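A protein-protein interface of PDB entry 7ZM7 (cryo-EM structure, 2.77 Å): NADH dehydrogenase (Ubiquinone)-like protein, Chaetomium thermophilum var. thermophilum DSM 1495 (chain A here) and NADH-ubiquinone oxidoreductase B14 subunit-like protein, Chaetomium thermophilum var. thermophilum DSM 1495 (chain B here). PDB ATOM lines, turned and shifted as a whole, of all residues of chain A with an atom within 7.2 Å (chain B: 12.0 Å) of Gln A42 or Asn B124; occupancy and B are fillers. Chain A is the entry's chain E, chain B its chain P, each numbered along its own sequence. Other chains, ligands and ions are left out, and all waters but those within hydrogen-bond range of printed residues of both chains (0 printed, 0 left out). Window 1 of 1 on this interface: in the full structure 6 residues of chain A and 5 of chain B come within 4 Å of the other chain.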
ATOM      1  N   ILE A  26       5.178  20.413 -23.543  1.00  0.00           N
ATOM      2  CA  ILE A  26       5.966  21.578 -23.177  1.00  0.00           C
ATOM      3  C   ILE A  26       5.051  22.761 -22.911  1.00  0.00           C
ATOM      4  O   ILE A  26       5.349  23.612 -22.079  1.00  0.00           O
ATOM      5  CB  ILE A  26       7.003  21.915 -24.264  1.00  0.00           C
ATOM      6  CG1 ILE A  26       6.377  21.789 -25.655  1.00  0.00           C
ATOM      7  CG2 ILE A  26       8.221  21.017 -24.136  1.00  0.00           C
ATOM      8  CD1 ILE A  26       7.277  22.246 -26.779  1.00  0.00           C
ATOM      9  N   SER A  27       3.936  22.801 -23.630  1.00  0.00           N
ATOM     10  CA  SER A  27       2.928  23.829 -23.440  1.00  0.00           C
ATOM     11  C   SER A  27       2.072  23.502 -22.224  1.00  0.00           C
ATOM     12  O   SER A  27       1.984  22.357 -21.783  1.00  0.00           O
ATOM     13  CB  SER A  27       2.058  23.953 -24.687  1.00  0.00           C
ATOM     14  OG  SER A  27       0.867  24.664 -24.427  1.00  0.00           O
ATOM     15  N   ASP A  28       1.448  24.535 -21.670  1.00  0.00           N
ATOM     16  CA  ASP A  28       0.602  24.342 -20.504  1.00  0.00           C
ATOM     17  C   ASP A  28      -0.824  23.978 -20.864  1.00  0.00           C
ATOM     18  O   ASP A  28      -1.588  23.586 -19.981  1.00  0.00           O
ATOM     19  CB  ASP A  28       0.608  25.598 -19.639  1.00  0.00           C
ATOM     20  CG  ASP A  28      -0.029  26.776 -20.327  1.00  0.00           C
ATOM     21  OD1 ASP A  28       0.358  27.082 -21.470  1.00  0.00           O
ATOM     22  OD2 ASP A  28      -0.922  27.395 -19.722  1.00  0.00           O
ATOM     23  N   ILE A  29      -1.199  24.088 -22.128  1.00  0.00           N
ATOM     24  CA  ILE A  29      -2.543  23.783 -22.586  1.00  0.00           C
ATOM     25  C   ILE A  29      -2.444  22.661 -23.594  1.00  0.00           C
ATOM     26  O   ILE A  29      -1.593  22.695 -24.485  1.00  0.00           O
ATOM     27  CB  ILE A  29      -3.231  25.002 -23.212  1.00  0.00           C
ATOM     28  CG1 ILE A  29      -3.109  26.217 -22.304  1.00  0.00           C
ATOM     29  CG2 ILE A  29      -4.661  24.674 -23.528  1.00  0.00           C
ATOM     30  CD1 ILE A  29      -3.059  27.508 -23.049  1.00  0.00           C
ATOM     31  N   ARG A  40      -2.448  22.071 -17.657  1.00  0.00           N
ATOM     32  CA  ARG A  40      -1.465  21.405 -16.828  1.00  0.00           C
ATOM     33  C   ARG A  40      -0.575  22.405 -16.102  1.00  0.00           C
ATOM     34  O   ARG A  40      -0.312  23.508 -16.583  1.00  0.00           O
ATOM     35  CB  ARG A  40      -0.610  20.466 -17.672  1.00  0.00           C
ATOM     36  CG  ARG A  40       0.479  21.136 -18.454  1.00  0.00           C
ATOM     37  CD  ARG A  40       1.198  20.176 -19.371  1.00  0.00           C
ATOM     38  NE  ARG A  40       0.426  19.877 -20.566  1.00  0.00           N
ATOM     39  CZ  ARG A  40       0.877  19.165 -21.593  1.00  0.00           C
ATOM     40  NH1 ARG A  40       0.092  18.942 -22.629  1.00  0.00           N
ATOM     41  NH2 ARG A  40       2.110  18.685 -21.589  1.00  0.00           N
ATOM     42  N   ILE A  41      -0.133  22.007 -14.916  1.00  0.00           N
ATOM     43  CA  ILE A  41       0.923  22.679 -14.174  1.00  0.00           C
ATOM     44  C   ILE A  41       2.128  21.760 -14.212  1.00  0.00           C
ATOM     45  O   ILE A  41       2.056  20.617 -13.757  1.00  0.00           O
ATOM     46  CB  ILE A  41       0.489  22.981 -12.732  1.00  0.00           C
ATOM     47  CG1 ILE A  41      -0.679  23.965 -12.736  1.00  0.00           C
ATOM     48  CG2 ILE A  41       1.654  23.495 -11.904  1.00  0.00           C
ATOM     49  CD1 ILE A  41      -1.522  23.908 -11.532  1.00  0.00           C
ATOM     50  N   GLN A  42       3.230  22.246 -14.758  1.00  0.00           N
ATOM     51  CA  GLN A  42       4.364  21.393 -15.093  1.00  0.00           C
ATOM     52  C   GLN A  42       5.363  21.397 -13.953  1.00  0.00           C
ATOM     53  O   GLN A  42       6.181  22.303 -13.831  1.00  0.00           O
ATOM     54  CB  GLN A  42       5.010  21.860 -16.384  1.00  0.00           C
ATOM     55  CG  GLN A  42       4.109  21.682 -17.561  1.00  0.00           C
ATOM     56  CD  GLN A  42       4.726  22.152 -18.827  1.00  0.00           C
ATOM     57  OE1 GLN A  42       5.830  22.683 -18.835  1.00  0.00           O
ATOM     58  NE2 GLN A  42       4.025  21.954 -19.924  1.00  0.00           N
ATOM     59  N   GLY A  43       5.301  20.374 -13.124  1.00  0.00           N
ATOM     60  CA  GLY A  43       6.279  20.186 -12.084  1.00  0.00           C
ATOM     61  C   GLY A  43       6.647  18.730 -11.949  1.00  0.00           C
ATOM     62  O   GLY A  43       6.915  18.058 -12.943  1.00  0.00           O
ATOM     63  N   GLY A  44       6.644  18.227 -10.727  1.00  0.00           N
ATOM     64  CA  GLY A  44       7.018  16.858 -10.478  1.00  0.00           C
ATOM     65  C   GLY A  44       5.886  16.021  -9.942  1.00  0.00           C
ATOM     66  O   GLY A  44       4.802  15.981 -10.526  1.00  0.00           O
ATOM     67  N   SER A  47       2.511  17.639  -8.926  1.00  0.00           N
ATOM     68  CA  SER A  47       1.989  18.556  -9.971  1.00  0.00           C
ATOM     69  C   SER A  47       0.708  18.063 -10.646  1.00  0.00           C
ATOM     70  O   SER A  47       0.090  17.157 -10.141  1.00  0.00           O
ATOM     71  CB  SER A  47       3.043  18.842 -10.989  1.00  0.00           C
ATOM     72  OG  SER A  47       3.246  17.726 -11.839  1.00  0.00           O
ATOM     73  N   LEU A  48       0.313  18.676 -11.754  1.00  0.00           N
ATOM     74  CA  LEU A  48      -0.901  18.362 -12.500  1.00  0.00           C
ATOM     75  C   LEU A  48      -0.523  18.169 -13.960  1.00  0.00           C
ATOM     76  O   LEU A  48      -0.493  19.125 -14.729  1.00  0.00           O
ATOM     77  CB  LEU A  48      -1.943  19.479 -12.345  1.00  0.00           C
ATOM     78  CG  LEU A  48      -2.367  19.900 -10.938  1.00  0.00           C
ATOM     79  CD1 LEU A  48      -3.527  20.835 -10.993  1.00  0.00           C
ATOM     80  CD2 LEU A  48      -2.709  18.702 -10.106  1.00  0.00           C
ATOM     81  N   GLY A  49      -0.236  16.930 -14.348  1.00  0.00           N
ATOM     82  CA  GLY A  49      -0.045  16.638 -15.756  1.00  0.00           C
ATOM     83  C   GLY A  49      -1.351  16.565 -16.522  1.00  0.00           C
ATOM     84  O   GLY A  49      -1.396  16.862 -17.718  1.00  0.00           O
ATOM     85  N   GLN A  73       5.556  13.040 -13.455  1.00  0.00           N
ATOM     86  CA  GLN A  73       5.202  14.400 -13.836  1.00  0.00           C
ATOM     87  C   GLN A  73       3.731  14.717 -13.586  1.00  0.00           C
ATOM     88  O   GLN A  73       3.209  15.665 -14.173  1.00  0.00           O
ATOM     89  CB  GLN A  73       5.545  14.646 -15.298  1.00  0.00           C
ATOM     90  CG  GLN A  73       4.735  13.802 -16.236  1.00  0.00           C
ATOM     91  CD  GLN A  73       5.101  13.977 -17.687  1.00  0.00           C
ATOM     92  OE1 GLN A  73       4.554  13.310 -18.569  1.00  0.00           O
ATOM     93  NE2 GLN A  73       6.019  14.893 -17.946  1.00  0.00           N
ATOM     94  N   TYR A 246       2.863  13.916 -26.509  1.00  0.00           N
ATOM     95  CA  TYR A 246       2.912  15.366 -26.373  1.00  0.00           C
ATOM     96  C   TYR A 246       2.853  16.094 -27.710  1.00  0.00           C
ATOM     97  O   TYR A 246       2.546  17.290 -27.740  1.00  0.00           O
ATOM     98  CB  TYR A 246       4.155  15.756 -25.593  1.00  0.00           C
ATOM     99  CG  TYR A 246       3.963  15.578 -24.118  1.00  0.00           C
ATOM    100  CD1 TYR A 246       2.701  15.660 -23.560  1.00  0.00           C
ATOM    101  CD2 TYR A 246       5.026  15.298 -23.286  1.00  0.00           C
ATOM    102  CE1 TYR A 246       2.510  15.494 -22.226  1.00  0.00           C
ATOM    103  CE2 TYR A 246       4.845  15.134 -21.944  1.00  0.00           C
ATOM    104  CZ  TYR A 246       3.584  15.234 -21.418  1.00  0.00           C
ATOM    105  OH  TYR A 246       3.393  15.074 -20.067  1.00  0.00           O
ATOM    106  N   LYS B 101      24.086  18.856 -12.519  1.00  0.00           N
ATOM    107  CA  LYS B 101      22.729  19.362 -12.671  1.00  0.00           C
ATOM    108  C   LYS B 101      22.145  19.039 -14.035  1.00  0.00           C
ATOM    109  O   LYS B 101      21.329  19.799 -14.563  1.00  0.00           O
ATOM    110  CB  LYS B 101      22.709  20.865 -12.396  1.00  0.00           C
ATOM    111  CG  LYS B 101      22.992  21.174 -10.940  1.00  0.00           C
ATOM    112  CD  LYS B 101      23.860  22.387 -10.783  1.00  0.00           C
ATOM    113  CE  LYS B 101      24.369  22.492  -9.363  1.00  0.00           C
ATOM    114  NZ  LYS B 101      25.257  21.370  -9.021  1.00  0.00           N
ATOM    115  N   HIS B 104      18.683  15.552 -13.808  1.00  0.00           N
ATOM    116  CA  HIS B 104      17.315  15.844 -13.441  1.00  0.00           C
ATOM    117  C   HIS B 104      16.470  15.419 -14.626  1.00  0.00           C
ATOM    118  O   HIS B 104      16.915  15.532 -15.771  1.00  0.00           O
ATOM    119  CB  HIS B 104      17.151  17.337 -13.156  1.00  0.00           C
ATOM    120  CG  HIS B 104      15.831  17.706 -12.561  1.00  0.00           C
ATOM    121  ND1 HIS B 104      14.634  17.507 -13.210  1.00  0.00           N
ATOM    122  CD2 HIS B 104      15.525  18.282 -11.379  1.00  0.00           C
ATOM    123  CE1 HIS B 104      13.647  17.929 -12.444  1.00  0.00           C
ATOM    124  NE2 HIS B 104      14.162  18.404 -11.328  1.00  0.00           N
ATOM    125  N   PHE B 105      15.272  14.902 -14.378  1.00  0.00           N
ATOM    126  CA  PHE B 105      14.543  14.468 -15.563  1.00  0.00           C
ATOM    127  C   PHE B 105      14.146  15.626 -16.458  1.00  0.00           C
ATOM    128  O   PHE B 105      13.722  15.388 -17.590  1.00  0.00           O
ATOM    129  CB  PHE B 105      13.321  13.619 -15.187  1.00  0.00           C
ATOM    130  CG  PHE B 105      12.158  14.386 -14.625  1.00  0.00           C
ATOM    131  CD1 PHE B 105      11.217  14.969 -15.444  1.00  0.00           C
ATOM    132  CD2 PHE B 105      11.964  14.442 -13.274  1.00  0.00           C
ATOM    133  CE1 PHE B 105      10.145  15.637 -14.918  1.00  0.00           C
ATOM    134  CE2 PHE B 105      10.892  15.093 -12.744  1.00  0.00           C
ATOM    135  CZ  PHE B 105       9.981  15.697 -13.564  1.00  0.00           C
ATOM    136  N   ARG B 106      14.260  16.858 -15.975  1.00  0.00           N
ATOM    137  CA  ARG B 106      14.141  18.045 -16.803  1.00  0.00           C
ATOM    138  C   ARG B 106      15.481  18.476 -17.371  1.00  0.00           C
ATOM    139  O   ARG B 106      15.516  19.226 -18.351  1.00  0.00           O
ATOM    140  CB  ARG B 106      13.563  19.206 -15.995  1.00  0.00           C
ATOM    141  CG  ARG B 106      12.246  18.953 -15.303  1.00  0.00           C
ATOM    142  CD  ARG B 106      11.104  18.938 -16.247  1.00  0.00           C
ATOM    143  NE  ARG B 106       9.837  18.937 -15.533  1.00  0.00           N
ATOM    144  CZ  ARG B 106       8.656  18.815 -16.116  1.00  0.00           C
ATOM    145  NH1 ARG B 106       8.572  18.674 -17.427  1.00  0.00           N
ATOM    146  NH2 ARG B 106       7.553  18.822 -15.388  1.00  0.00           N
ATOM    147  N   GLY B 107      16.567  18.034 -16.774  1.00  0.00           N
ATOM    148  CA  GLY B 107      17.869  18.259 -17.328  1.00  0.00           C
ATOM    149  C   GLY B 107      18.459  19.590 -16.929  1.00  0.00           C
ATOM    150  O   GLY B 107      17.944  20.328 -16.086  1.00  0.00           O
ATOM    151  N   GLU B 108      19.593  19.889 -17.566  1.00  0.00           N
ATOM    152  CA  GLU B 108      20.251  21.172 -17.377  1.00  0.00           C
ATOM    153  C   GLU B 108      19.343  22.327 -17.767  1.00  0.00           C
ATOM    154  O   GLU B 108      19.284  23.329 -17.049  1.00  0.00           O
ATOM    155  CB  GLU B 108      21.536  21.210 -18.204  1.00  0.00           C
ATOM    156  CG  GLU B 108      22.382  22.452 -18.021  1.00  0.00           C
ATOM    157  CD  GLU B 108      23.035  22.509 -16.657  1.00  0.00           C
ATOM    158  OE1 GLU B 108      23.236  21.436 -16.052  1.00  0.00           O
ATOM    159  OE2 GLU B 108      23.357  23.623 -16.197  1.00  0.00           O
ATOM    160  N   LYS B 109      18.620  22.195 -18.872  1.00  0.00           N
ATOM    161  CA  LYS B 109      17.683  23.216 -19.326  1.00  0.00           C
ATOM    162  C   LYS B 109      16.500  23.217 -18.368  1.00  0.00           C
ATOM    163  O   LYS B 109      15.547  22.453 -18.536  1.00  0.00           O
ATOM    164  CB  LYS B 109      17.257  22.939 -20.763  1.00  0.00           C
ATOM    165  CG  LYS B 109      16.257  23.922 -21.342  1.00  0.00           C
ATOM    166  CD  LYS B 109      14.873  23.300 -21.444  1.00  0.00           C
ATOM    167  CE  LYS B 109      14.894  22.073 -22.339  1.00  0.00           C
ATOM    168  NZ  LYS B 109      13.563  21.415 -22.421  1.00  0.00           N
ATOM    169  N   ARG B 110      16.568  24.065 -17.343  1.00  0.00           N
ATOM    170  CA  ARG B 110      15.492  24.161 -16.372  1.00  0.00           C
ATOM    171  C   ARG B 110      14.985  25.571 -16.135  1.00  0.00           C
ATOM    172  O   ARG B 110      13.872  25.723 -15.620  1.00  0.00           O
ATOM    173  CB  ARG B 110      15.909  23.549 -15.032  1.00  0.00           C
ATOM    174  CG  ARG B 110      15.473  22.113 -14.914  1.00  0.00           C
ATOM    175  CD  ARG B 110      15.742  21.592 -13.553  1.00  0.00           C
ATOM    176  NE  ARG B 110      17.128  21.196 -13.396  1.00  0.00           N
ATOM    177  CZ  ARG B 110      17.758  21.182 -12.236  1.00  0.00           C
ATOM    178  NH1 ARG B 110      17.126  21.546 -11.136  1.00  0.00           N
ATOM    179  NH2 ARG B 110      19.017  20.794 -12.182  1.00  0.00           N
ATOM    180  N   LEU B 111      15.741  26.571 -16.458  1.00  0.00           N
ATOM    181  CA  LEU B 111      15.165  27.885 -16.613  1.00  0.00           C
ATOM    182  C   LEU B 111      14.740  28.078 -18.057  1.00  0.00           C
ATOM    183  O   LEU B 111      15.284  27.439 -18.956  1.00  0.00           O
ATOM    184  CB  LEU B 111      16.168  28.974 -16.235  1.00  0.00           C
ATOM    185  CG  LEU B 111      16.445  29.247 -14.757  1.00  0.00           C
ATOM    186  CD1 LEU B 111      17.214  30.529 -14.604  1.00  0.00           C
ATOM    187  CD2 LEU B 111      15.167  29.308 -13.967  1.00  0.00           C
ATOM    188  N   PRO B 112      13.760  28.929 -18.324  1.00  0.00           N
ATOM    189  CA  PRO B 112      13.430  29.248 -19.713  1.00  0.00           C
ATOM    190  C   PRO B 112      14.572  29.990 -20.394  1.00  0.00           C
ATOM    191  O   PRO B 112      15.297  30.763 -19.767  1.00  0.00           O
ATOM    192  CB  PRO B 112      12.181  30.119 -19.581  1.00  0.00           C
ATOM    193  CG  PRO B 112      12.236  30.642 -18.238  1.00  0.00           C
ATOM    194  CD  PRO B 112      12.874  29.624 -17.384  1.00  0.00           C
ATOM    195  N   SER B 113      14.723  29.748 -21.696  1.00  0.00           N
ATOM    196  CA  SER B 113      15.874  30.271 -22.423  1.00  0.00           C
ATOM    197  C   SER B 113      15.784  31.776 -22.615  1.00  0.00           C
ATOM    198  O   SER B 113      16.783  32.490 -22.478  1.00  0.00           O
ATOM    199  CB  SER B 113      15.993  29.580 -23.777  1.00  0.00           C
ATOM    200  OG  SER B 113      16.737  30.377 -24.681  1.00  0.00           O
ATOM    201  N   ASN B 114      14.602  32.269 -22.946  1.00  0.00           N
ATOM    202  CA  ASN B 114      14.394  33.666 -23.229  1.00  0.00           C
ATOM    203  C   ASN B 114      12.978  34.004 -22.787  1.00  0.00           C
ATOM    204  O   ASN B 114      12.329  33.213 -22.100  1.00  0.00           O
ATOM    205  CB  ASN B 114      14.650  33.929 -24.714  1.00  0.00           C
ATOM    206  CG  ASN B 114      13.640  33.254 -25.598  1.00  0.00           C
ATOM    207  OD1 ASN B 114      13.581  32.035 -25.679  1.00  0.00           O
ATOM    208  ND2 ASN B 114      12.819  34.056 -26.254  1.00  0.00           N
ATOM    209  N   PHE B 115      12.479  35.169 -23.186  1.00  0.00           N
ATOM    210  CA  PHE B 115      11.132  35.525 -22.765  1.00  0.00           C
ATOM    211  C   PHE B 115      10.086  34.601 -23.379  1.00  0.00           C
ATOM    212  O   PHE B 115       9.251  34.049 -22.662  1.00  0.00           O
ATOM    213  CB  PHE B 115      10.816  36.978 -23.097  1.00  0.00           C
ATOM    214  CG  PHE B 115       9.454  37.378 -22.678  1.00  0.00           C
ATOM    215  CD1 PHE B 115       9.218  37.801 -21.391  1.00  0.00           C
ATOM    216  CD2 PHE B 115       8.387  37.280 -23.553  1.00  0.00           C
ATOM    217  CE1 PHE B 115       7.958  38.137 -20.994  1.00  0.00           C
ATOM    218  CE2 PHE B 115       7.125  37.602 -23.152  1.00  0.00           C
ATOM    219  CZ  PHE B 115       6.913  38.036 -21.876  1.00  0.00           C
ATOM    220  N   ILE B 116      10.107  34.413 -24.698  1.00  0.00           N
ATOM    221  CA  ILE B 116       8.946  33.822 -25.367  1.00  0.00           C
ATOM    222  C   ILE B 116       8.794  32.345 -25.021  1.00  0.00           C
ATOM    223  O   ILE B 116       7.674  31.853 -24.859  1.00  0.00           O
ATOM    224  CB  ILE B 116       9.009  34.049 -26.889  1.00  0.00           C
ATOM    225  CG1 ILE B 116       7.642  33.803 -27.510  1.00  0.00           C
ATOM    226  CG2 ILE B 116       9.990  33.123 -27.549  1.00  0.00           C
ATOM    227  CD1 ILE B 116       6.592  34.767 -27.065  1.00  0.00           C
ATOM    228  N   THR B 117       9.898  31.608 -24.909  1.00  0.00           N
ATOM    229  CA  THR B 117       9.774  30.182 -24.645  1.00  0.00           C
ATOM    230  C   THR B 117       9.287  29.913 -23.232  1.00  0.00           C
ATOM    231  O   THR B 117       8.593  28.919 -22.997  1.00  0.00           O
ATOM    232  CB  THR B 117      11.098  29.473 -24.901  1.00  0.00           C
ATOM    233  OG1 THR B 117      12.107  29.992 -24.030  1.00  0.00           O
ATOM    234  CG2 THR B 117      11.520  29.652 -26.344  1.00  0.00           C
ATOM    235  N   GLY B 118       9.639  30.774 -22.284  1.00  0.00           N
ATOM    236  CA  GLY B 118       9.079  30.663 -20.955  1.00  0.00           C
ATOM    237  C   GLY B 118       7.662  31.160 -20.852  1.00  0.00           C
ATOM    238  O   GLY B 118       6.934  30.764 -19.943  1.00  0.00           O
ATOM    239  N   PHE B 119       7.252  32.040 -21.757  1.00  0.00           N
ATOM    240  CA  PHE B 119       5.860  32.461 -21.782  1.00  0.00           C
ATOM    241  C   PHE B 119       4.966  31.350 -22.306  1.00  0.00           C
ATOM    242  O   PHE B 119       3.858  31.145 -21.801  1.00  0.00           O
ATOM    243  CB  PHE B 119       5.706  33.723 -22.624  1.00  0.00           C
ATOM    244  CG  PHE B 119       4.293  34.184 -22.758  1.00  0.00           C
ATOM    245  CD1 PHE B 119       3.731  35.002 -21.809  1.00  0.00           C
ATOM    246  CD2 PHE B 119       3.523  33.789 -23.826  1.00  0.00           C
ATOM    247  CE1 PHE B 119       2.447  35.414 -21.922  1.00  0.00           C
ATOM    248  CE2 PHE B 119       2.229  34.206 -23.931  1.00  0.00           C
ATOM    249  CZ  PHE B 119       1.695  35.018 -22.972  1.00  0.00           C
ATOM    250  N   LEU B 120       5.408  30.646 -23.344  1.00  0.00           N
ATOM    251  CA  LEU B 120       4.507  29.628 -23.951  1.00  0.00           C
ATOM    252  C   LEU B 120       4.413  28.403 -23.040  1.00  0.00           C
ATOM    253  O   LEU B 120       3.437  27.660 -23.167  1.00  0.00           O
ATOM    254  CB  LEU B 120       4.996  29.286 -25.359  1.00  0.00           C
ATOM    255  CG  LEU B 120       4.960  30.444 -26.353  1.00  0.00           C
ATOM    256  CD1 LEU B 120       5.546  30.031 -27.690  1.00  0.00           C
ATOM    257  CD2 LEU B 120       3.542  30.961 -26.524  1.00  0.00           C
ATOM    258  N   GLU B 121       5.358  28.245 -22.112  1.00  0.00           N
ATOM    259  CA  GLU B 121       5.383  27.091 -21.174  1.00  0.00           C
ATOM    260  C   GLU B 121       4.906  27.487 -19.774  1.00  0.00           C
ATOM    261  O   GLU B 121       5.010  26.629 -18.880  1.00  0.00           O
ATOM    262  CB  GLU B 121       6.811  26.553 -21.087  1.00  0.00           C
ATOM    263  CG  GLU B 121       7.339  26.051 -22.416  1.00  0.00           C
ATOM    264  CD  GLU B 121       8.776  25.563 -22.392  1.00  0.00           C
ATOM    265  OE1 GLU B 121       9.443  25.748 -21.355  1.00  0.00           O
ATOM    266  OE2 GLU B 121       9.223  24.998 -23.408  1.00  0.00           O
ATOM    267  N   GLY B 122       4.457  28.726 -19.566  1.00  0.00           N
ATOM    268  CA  GLY B 122       4.040  29.197 -18.223  1.00  0.00           C
ATOM    269  C   GLY B 122       5.194  29.311 -17.237  1.00  0.00           C
ATOM    270  O   GLY B 122       5.166  28.584 -16.231  1.00  0.00           O
ATOM    271  N   ARG B 123       6.162  30.190 -17.489  1.00  0.00           N
ATOM    272  CA  ARG B 123       7.371  30.378 -16.633  1.00  0.00           C
ATOM    273  C   ARG B 123       8.192  29.084 -16.506  1.00  0.00           C
ATOM    274  O   ARG B 123       8.704  28.865 -15.392  1.00  0.00           O
ATOM    275  CB  ARG B 123       7.020  31.054 -15.304  1.00  0.00           C
ATOM    276  CG  ARG B 123       8.085  32.016 -14.797  1.00  0.00           C
ATOM    277  CD  ARG B 123       7.746  32.780 -13.531  1.00  0.00           C
ATOM    278  NE  ARG B 123       7.696  31.966 -12.325  1.00  0.00           N
ATOM    279  CZ  ARG B 123       6.581  31.631 -11.687  1.00  0.00           C
ATOM    280  NH1 ARG B 123       5.411  32.049 -12.134  1.00  0.00           N
ATOM    281  NH2 ARG B 123       6.642  30.889 -10.598  1.00  0.00           N
ATOM    282  N   ASN B 124       8.330  28.291 -17.578  1.00  0.00           N
ATOM    283  CA  ASN B 124       9.081  26.993 -17.581  1.00  0.00           C
ATOM    284  C   ASN B 124       8.195  25.814 -17.149  1.00  0.00           C
ATOM    285  O   ASN B 124       8.458  24.698 -17.584  1.00  0.00           O
ATOM    286  CB  ASN B 124      10.455  26.993 -16.897  1.00  0.00           C
ATOM    287  CG  ASN B 124      11.362  25.935 -17.485  1.00  0.00           C
ATOM    288  OD1 ASN B 124      11.534  24.866 -16.908  1.00  0.00           O
ATOM    289  ND2 ASN B 124      11.914  26.208 -18.655  1.00  0.00           N
ATOM    290  OXT ASN B 124       7.249  26.045 -16.393  1.00  0.00           O
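Gln A42 touches just these residues of chain B: Arg B106 (3.7 Å) and Asn B124 (3.5 Å). Asn B124 touches just one residue of chain A: Gln A42. Of chain B, only Leu B120 (3.9 Å) comes within 4 Å of Ser A27. Of the printed residues of chain B, Asp A28 touches Leu B120. Gly A43 touches just these residues of chain B: Phe B105 (3.9 Å) and Arg B106 (2.6 Å). No residue of chain B comes within 4 Å of Gly A44. No residue of chain B comes within 4 Å of Ser A47. No residue of chain B comes within 4 Å of Gly A49. Of the printed residues of chain A, Phe B105 touches Gly A43 (3.9 Å). Of the printed residues of chain A, Arg B106 touches Gln A42 (3.7 Å) and Gly A43 (2.6 Å). Of the printed residues of chain A, Leu B120 touches Ser A27 and Asp A28. The nearest residue of chain B that does not touch Gln A42 is Glu B121 (4.03 Å). The nearest residue of chain A that does not touch Asn B124 is Ile A26 (5.6 Å).
Ile A26 touches Glu B121. O of Leu B120 touches CA of Ser A27 (3.9 Å). O of Leu B120 touches OD1 of Asp A28 (3.6 Å). NH2 of Arg B106 touches C of Gln A42, 3.7 Å away. OE1 of Gln A42 touches O of Asn B124 (3.5 Å). Gly A43 touches Phe B105 (O to CZ, 3.9 Å).
Of the 14 printed residues of chain A, 5 touch a printed residue of chain B. Hydrophobic or aromatic side chains of chain A within 4 Å of the printed part of chain B: Ile A26. Among the printed residues, 7 pairs touch across the chains. Among the printed residues, no Asp or Glu carboxylate lies within 4 Å of a Lys or Arg side-chain nitrogen of the other chain.
The guanidinium group of Arg B106 is in hydrogen-bond range of the backbone carbonyl oxygen of Gly A43 (2.6 Å).
OG of Ser A27 lies within hydrogen-bond range of N of Ile A29, at 3.1 Å. The backbone carbonyl oxygen of Ser A27 sits at hydrogen-bond distance from the guanidinium group of Arg A40, 3.2 Å away. O of Ser A27 lies within hydrogen-bond range of NE2 of Gln A42. The backbone NH (N) of Arg A40 is in hydrogen-bond range of the backbone carbonyl oxygen (O) of Asp A28 (2.9 Å). A ring nitrogen (ND1) of His B104 is in hydrogen-bond range of the backbone NH (N) of Arg B106 (2.9 Å). O of Arg B110 lies close to OD1 of Asn B124, 2.8 Å away.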
